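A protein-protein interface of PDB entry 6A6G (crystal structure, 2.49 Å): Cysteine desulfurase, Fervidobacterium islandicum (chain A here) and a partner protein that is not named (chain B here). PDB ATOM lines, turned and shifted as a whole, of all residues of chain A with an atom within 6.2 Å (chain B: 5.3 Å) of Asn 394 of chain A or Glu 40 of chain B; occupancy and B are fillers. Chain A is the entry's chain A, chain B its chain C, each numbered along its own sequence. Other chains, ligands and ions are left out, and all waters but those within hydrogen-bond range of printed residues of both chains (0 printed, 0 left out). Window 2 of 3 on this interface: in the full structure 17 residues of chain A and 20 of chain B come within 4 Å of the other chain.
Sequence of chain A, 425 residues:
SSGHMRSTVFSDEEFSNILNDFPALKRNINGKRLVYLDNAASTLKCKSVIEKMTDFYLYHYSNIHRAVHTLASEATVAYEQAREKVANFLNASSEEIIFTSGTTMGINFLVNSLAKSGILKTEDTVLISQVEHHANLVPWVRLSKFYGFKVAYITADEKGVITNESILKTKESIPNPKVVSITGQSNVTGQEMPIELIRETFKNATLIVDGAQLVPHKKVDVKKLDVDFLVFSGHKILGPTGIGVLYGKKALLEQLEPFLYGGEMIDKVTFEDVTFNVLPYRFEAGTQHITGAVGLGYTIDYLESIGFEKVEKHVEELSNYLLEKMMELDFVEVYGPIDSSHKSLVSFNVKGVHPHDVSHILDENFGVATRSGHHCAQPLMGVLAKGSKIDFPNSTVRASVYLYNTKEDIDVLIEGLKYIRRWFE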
ATOM      1  N   ASN A 349      14.287  29.562  -6.391  1.00  0.00           N
ATOM      2  CA  ASN A 349      15.605  29.539  -7.025  1.00  0.00           C
ATOM      3  C   ASN A 349      15.476  30.213  -8.388  1.00  0.00           C
ATOM      4  O   ASN A 349      14.421  30.209  -8.979  1.00  0.00           O
ATOM      5  CB  ASN A 349      16.156  28.118  -7.161  1.00  0.00           C
ATOM      6  CG  ASN A 349      16.948  27.652  -5.946  1.00  0.00           C
ATOM      7  OD1 ASN A 349      17.933  28.298  -5.525  1.00  0.00           O
ATOM      8  ND2 ASN A 349      16.561  26.465  -5.403  1.00  0.00           N
ATOM      9  N   HIS A 354      23.042  30.049  -8.830  1.00  0.00           N
ATOM     10  CA  HIS A 354      23.141  29.625  -7.429  1.00  0.00           C
ATOM     11  C   HIS A 354      22.664  30.711  -6.454  1.00  0.00           C
ATOM     12  O   HIS A 354      22.901  31.912  -6.666  1.00  0.00           O
ATOM     13  CB  HIS A 354      24.583  29.226  -7.098  1.00  0.00           C
ATOM     14  CG  HIS A 354      24.735  28.472  -5.814  1.00  0.00           C
ATOM     15  ND1 HIS A 354      24.834  29.096  -4.590  1.00  0.00           N
ATOM     16  CD2 HIS A 354      24.883  27.147  -5.567  1.00  0.00           C
ATOM     17  CE1 HIS A 354      25.000  28.184  -3.639  1.00  0.00           C
ATOM     18  NE2 HIS A 354      25.052  26.995  -4.204  1.00  0.00           N
ATOM     19  N   GLY A 373      20.693  29.734   1.036  1.00  0.00           N
ATOM     20  CA  GLY A 373      21.226  28.553   1.672  1.00  0.00           C
ATOM     21  C   GLY A 373      20.146  27.572   2.088  1.00  0.00           C
ATOM     22  O   GLY A 373      19.138  27.472   1.432  1.00  0.00           O
ATOM     23  N   HIS A 374      20.353  26.870   3.201  1.00  0.00           N
ATOM     24  CA  HIS A 374      19.427  25.821   3.673  1.00  0.00           C
ATOM     25  C   HIS A 374      18.325  26.375   4.561  1.00  0.00           C
ATOM     26  O   HIS A 374      17.365  25.663   4.856  1.00  0.00           O
ATOM     27  CB  HIS A 374      20.168  24.730   4.479  1.00  0.00           C
ATOM     28  CG  HIS A 374      21.290  24.085   3.731  1.00  0.00           C
ATOM     29  ND1 HIS A 374      21.090  23.307   2.607  1.00  0.00           N
ATOM     30  CD2 HIS A 374      22.632  24.129   3.921  1.00  0.00           C
ATOM     31  CE1 HIS A 374      22.257  22.890   2.143  1.00  0.00           C
ATOM     32  NE2 HIS A 374      23.209  23.374   2.924  1.00  0.00           N
ATOM     33  N   MET A 381      15.371  20.531   2.333  1.00  0.00           N
ATOM     34  CA  MET A 381      16.026  20.742   1.042  1.00  0.00           C
ATOM     35  C   MET A 381      15.998  19.467   0.193  1.00  0.00           C
ATOM     36  O   MET A 381      15.773  19.564  -0.998  1.00  0.00           O
ATOM     37  CB  MET A 381      17.482  21.232   1.205  1.00  0.00           C
ATOM     38  CG  MET A 381      17.643  22.599   1.860  1.00  0.00           C
ATOM     39  SD  MET A 381      16.805  23.924   0.971  1.00  0.00           S
ATOM     40  CE  MET A 381      15.520  24.462   2.084  1.00  0.00           C
ATOM     41  N   GLY A 382      16.205  18.287   0.789  1.00  0.00           N
ATOM     42  CA  GLY A 382      16.127  17.001   0.046  1.00  0.00           C
ATOM     43  C   GLY A 382      14.726  16.669  -0.468  1.00  0.00           C
ATOM     44  O   GLY A 382      14.552  16.071  -1.541  1.00  0.00           O
ATOM     45  N   ALA A 385      14.175  18.963  -3.332  1.00  0.00           N
ATOM     46  CA  ALA A 385      15.015  18.432  -4.419  1.00  0.00           C
ATOM     47  C   ALA A 385      14.225  17.458  -5.256  1.00  0.00           C
ATOM     48  O   ALA A 385      14.172  17.584  -6.474  1.00  0.00           O
ATOM     49  CB  ALA A 385      16.281  17.758  -3.879  1.00  0.00           C
ATOM     50  N   PHE A 392      18.729  21.433  -9.139  1.00  0.00           N
ATOM     51  CA  PHE A 392      18.454  21.971  -7.833  1.00  0.00           C
ATOM     52  C   PHE A 392      19.741  22.068  -7.026  1.00  0.00           C
ATOM     53  O   PHE A 392      20.429  21.067  -6.872  1.00  0.00           O
ATOM     54  CB  PHE A 392      17.394  21.122  -7.128  1.00  0.00           C
ATOM     55  CG  PHE A 392      16.975  21.665  -5.797  1.00  0.00           C
ATOM     56  CD1 PHE A 392      16.197  22.798  -5.721  1.00  0.00           C
ATOM     57  CD2 PHE A 392      17.366  21.038  -4.619  1.00  0.00           C
ATOM     58  CE1 PHE A 392      15.818  23.306  -4.490  1.00  0.00           C
ATOM     59  CE2 PHE A 392      16.982  21.540  -3.389  1.00  0.00           C
ATOM     60  CZ  PHE A 392      16.203  22.671  -3.326  1.00  0.00           C
ATOM     61  N   PRO A 393      20.055  23.268  -6.492  1.00  0.00           N
ATOM     62  CA  PRO A 393      21.338  23.548  -5.809  1.00  0.00           C
ATOM     63  C   PRO A 393      21.455  23.184  -4.310  1.00  0.00           C
ATOM     64  O   PRO A 393      22.392  23.618  -3.607  1.00  0.00           O
ATOM     65  CB  PRO A 393      21.516  25.038  -6.040  1.00  0.00           C
ATOM     66  CG  PRO A 393      20.131  25.583  -6.246  1.00  0.00           C
ATOM     67  CD  PRO A 393      19.284  24.490  -6.775  1.00  0.00           C
ATOM     68  N   ASN A 394      20.523  22.360  -3.846  1.00  0.00           N
ATOM     69  CA  ASN A 394      20.414  21.985  -2.446  1.00  0.00           C
ATOM     70  C   ASN A 394      20.425  23.228  -1.536  1.00  0.00           C
ATOM     71  O   ASN A 394      20.998  23.260  -0.449  1.00  0.00           O
ATOM     72  CB  ASN A 394      21.450  20.925  -2.108  1.00  0.00           C
ATOM     73  CG  ASN A 394      21.291  19.659  -2.984  1.00  0.00           C
ATOM     74  OD1 ASN A 394      20.200  19.361  -3.483  1.00  0.00           O
ATOM     75  ND2 ASN A 394      22.380  18.925  -3.173  1.00  0.00           N
ATOM     76  N   SER A 395      19.706  24.234  -2.012  1.00  0.00           N
ATOM     77  CA  SER A 395      19.523  25.481  -1.326  1.00  0.00           C
ATOM     78  C   SER A 395      18.608  26.334  -2.163  1.00  0.00           C
ATOM     79  O   SER A 395      18.307  26.013  -3.309  1.00  0.00           O
ATOM     80  CB  SER A 395      20.845  26.212  -1.095  1.00  0.00           C
ATOM     81  OG  SER A 395      21.512  26.307  -2.313  1.00  0.00           O
ATOM     82  N   THR A 396      18.151  27.414  -1.556  1.00  0.00           N
ATOM     83  CA  THR A 396      17.248  28.333  -2.168  1.00  0.00           C
ATOM     84  C   THR A 396      17.608  29.724  -1.664  1.00  0.00           C
ATOM     85  O   THR A 396      18.384  29.896  -0.699  1.00  0.00           O
ATOM     86  CB  THR A 396      15.767  28.001  -1.835  1.00  0.00           C
ATOM     87  OG1 THR A 396      15.416  28.545  -0.568  1.00  0.00           O
ATOM     88  CG2 THR A 396      15.494  26.501  -1.792  1.00  0.00           C
ATOM     89  N   GLY B  38      25.706  25.658   1.705  1.00  0.00           N
ATOM     90  CA  GLY B  38      25.149  24.898   0.570  1.00  0.00           C
ATOM     91  C   GLY B  38      25.913  24.987  -0.739  1.00  0.00           C
ATOM     92  O   GLY B  38      25.353  24.776  -1.823  1.00  0.00           O
ATOM     93  N   ASP B  39      27.189  25.320  -0.642  1.00  0.00           N
ATOM     94  CA  ASP B  39      28.131  25.123  -1.725  1.00  0.00           C
ATOM     95  C   ASP B  39      28.722  23.752  -1.460  1.00  0.00           C
ATOM     96  O   ASP B  39      29.129  23.488  -0.356  1.00  0.00           O
ATOM     97  CB  ASP B  39      29.302  26.153  -1.664  1.00  0.00           C
ATOM     98  CG  ASP B  39      29.003  27.482  -2.336  1.00  0.00           C
ATOM     99  OD1 ASP B  39      28.116  27.552  -3.199  1.00  0.00           O
ATOM    100  OD2 ASP B  39      29.694  28.475  -2.011  1.00  0.00           O
ATOM    101  N   GLU B  40      28.856  22.911  -2.467  1.00  0.00           N
ATOM    102  CA  GLU B  40      29.383  21.575  -2.239  1.00  0.00           C
ATOM    103  C   GLU B  40      30.526  21.276  -3.194  1.00  0.00           C
ATOM    104  O   GLU B  40      30.441  21.551  -4.395  1.00  0.00           O
ATOM    105  CB  GLU B  40      28.276  20.531  -2.448  1.00  0.00           C
ATOM    106  CG  GLU B  40      26.995  20.788  -1.654  1.00  0.00           C
ATOM    107  CD  GLU B  40      25.739  20.171  -2.274  1.00  0.00           C
ATOM    108  OE1 GLU B  40      25.729  19.877  -3.512  1.00  0.00           O
ATOM    109  OE2 GLU B  40      24.751  19.997  -1.506  1.00  0.00           O
ATOM    110  N   VAL B  41      31.601  20.716  -2.654  1.00  0.00           N
ATOM    111  CA  VAL B  41      32.653  20.166  -3.479  1.00  0.00           C
ATOM    112  C   VAL B  41      33.015  18.782  -2.971  1.00  0.00           C
ATOM    113  O   VAL B  41      33.135  18.554  -1.762  1.00  0.00           O
ATOM    114  CB  VAL B  41      33.894  21.088  -3.565  1.00  0.00           C
ATOM    115  CG1 VAL B  41      34.635  21.166  -2.250  1.00  0.00           C
ATOM    116  CG2 VAL B  41      34.826  20.589  -4.649  1.00  0.00           C
ATOM    117  N   THR B  42      33.122  17.842  -3.899  1.00  0.00           N
ATOM    118  CA  THR B  42      33.701  16.554  -3.592  1.00  0.00           C
ATOM    119  C   THR B  42      34.817  16.396  -4.582  1.00  0.00           C
ATOM    120  O   THR B  42      34.591  16.484  -5.785  1.00  0.00           O
ATOM    121  CB  THR B  42      32.688  15.397  -3.706  1.00  0.00           C
ATOM    122  OG1 THR B  42      31.716  15.524  -2.662  1.00  0.00           O
ATOM    123  CG2 THR B  42      33.380  14.064  -3.535  1.00  0.00           C
ATOM    124  N   GLU B  58      32.612  17.200  -8.147  1.00  0.00           N
ATOM    125  CA  GLU B  58      31.178  17.400  -8.310  1.00  0.00           C
ATOM    126  C   GLU B  58      30.654  18.236  -7.164  1.00  0.00           C
ATOM    127  O   GLU B  58      31.284  18.353  -6.098  1.00  0.00           O
ATOM    128  CB  GLU B  58      30.432  16.065  -8.327  1.00  0.00           C
ATOM    129  CG  GLU B  58      30.746  15.187  -9.531  1.00  0.00           C
ATOM    130  CD  GLU B  58      30.308  13.737  -9.343  1.00  0.00           C
ATOM    131  OE1 GLU B  58      30.481  13.180  -8.225  1.00  0.00           O
ATOM    132  OE2 GLU B  58      29.806  13.152 -10.331  1.00  0.00           O
ATOM    133  N   GLY B  59      29.480  18.805  -7.399  1.00  0.00           N
ATOM    134  CA  GLY B  59      28.777  19.551  -6.385  1.00  0.00           C
ATOM    135  C   GLY B  59      28.156  20.801  -6.960  1.00  0.00           C
ATOM    136  O   GLY B  59      28.707  21.425  -7.879  1.00  0.00           O
ATOM    137  N   HIS B  60      27.009  21.164  -6.413  1.00  0.00           N
ATOM    138  CA  HIS B  60      26.391  22.423  -6.727  1.00  0.00           C
ATOM    139  C   HIS B  60      27.138  23.527  -5.972  1.00  0.00           C
ATOM    140  O   HIS B  60      27.478  23.371  -4.799  1.00  0.00           O
ATOM    141  CB  HIS B  60      24.897  22.383  -6.417  1.00  0.00           C
ATOM    142  CG  HIS B  60      24.163  21.364  -7.233  1.00  0.00           C
ATOM    143  ND1 HIS B  60      23.857  20.107  -6.754  1.00  0.00           N
ATOM    144  CD2 HIS B  60      23.724  21.397  -8.515  1.00  0.00           C
ATOM    145  CE1 HIS B  60      23.233  19.421  -7.694  1.00  0.00           C
ATOM    146  NE2 HIS B  60      23.141  20.179  -8.774  1.00  0.00           N
ATOM    147  N   GLY B  61      27.424  24.616  -6.685  1.00  0.00           N
ATOM    148  CA  GLY B  61      28.190  25.708  -6.141  1.00  0.00           C
ATOM    149  C   GLY B  61      27.976  26.985  -6.907  1.00  0.00           C
ATOM    150  O   GLY B  61      27.814  27.004  -8.115  1.00  0.00           O
ATOM    151  N   LEU B 126      36.323  27.070   0.364  1.00  0.00           N
ATOM    152  CA  LEU B 126      35.740  25.720   0.362  1.00  0.00           C
ATOM    153  C   LEU B 126      36.596  24.665  -0.336  1.00  0.00           C
ATOM    154  O   LEU B 126      36.928  23.682   0.283  1.00  0.00           O
ATOM    155  CB  LEU B 126      34.306  25.685  -0.191  1.00  0.00           C
ATOM    156  CG  LEU B 126      33.748  24.255  -0.338  1.00  0.00           C
ATOM    157  CD1 LEU B 126      33.656  23.607   1.038  1.00  0.00           C
ATOM    158  CD2 LEU B 126      32.405  24.213  -1.054  1.00  0.00           C
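The side-chain amide nitrogen (ND2) of Asn 394 of chain A is in hydrogen-bond range of the side-chain carboxylate (OE2) of Glu 40 of chain B (3.1 Å).
NE2 of His 354 of chain A is in hydrogen-bond range of O of Gly 38 of chain B (3.3 Å).
The backbone carbonyl oxygen (O) of Phe 392 of chain A lies close to a ring nitrogen (NE2) of His 60 of chain B, at 3.4 Å.
A ring nitrogen (NE2) of His 354 of chain A sits close to the side-chain carboxylate (OD1) of Asp 39 of chain B, at 3.3 Å.
The side-chain hydroxyl of Ser 395 of chain A lies within hydrogen-bond range of the backbone carbonyl oxygen of Pro 393 of chain A (3.1 Å).
The backbone carbonyl oxygen (O) of Asn 394 of chain A sits close to a ring nitrogen (ND1) of His 374 of chain A, at 3.1 Å.
The backbone carbonyl oxygen (O) of His 60 of chain B is in hydrogen-bond range of the backbone NH (N) of Glu 40 of chain B, at 2.7 Å.
C of Gly 61 of chain B touches CD2 of His 354 of chain A (3.4 Å).
CA of Gly 38 of chain B touches NE2 of His 374 of chain A (3.4 Å).
Gly 38 of chain B touches Pro 393 of chain A (O to O, 3.6 Å).
Pro 393 of chain A touches His 60 of chain B.
Printed residues of chain B within 4 Å of His 374 of chain A: Gly 38 (3.4 Å).
Of the printed residues of chain B, Pro 393 of chain A touches Gly 38 and His 60.
Asn 394 of chain A touches one residue of chain B.
Of chain A, only Asn 394 comes within 4 Å of Glu 40 of chain B.
The nearest residue of chain B that does not touch Asn 394 of chain A is His 60 of chain B (4.05 Å).
Hydrophobic or aromatic side chains of chain B within 4 Å of the printed part of chain A: His 60.
Printed residues of chain A that touch a printed residue of chain B: His 354, His 374, Phe 392, Pro 393 and Asn 394.
Among the printed residues, no Asp or Glu carboxylate lies within 4 Å of a Lys or Arg side-chain nitrogen of the other chain.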
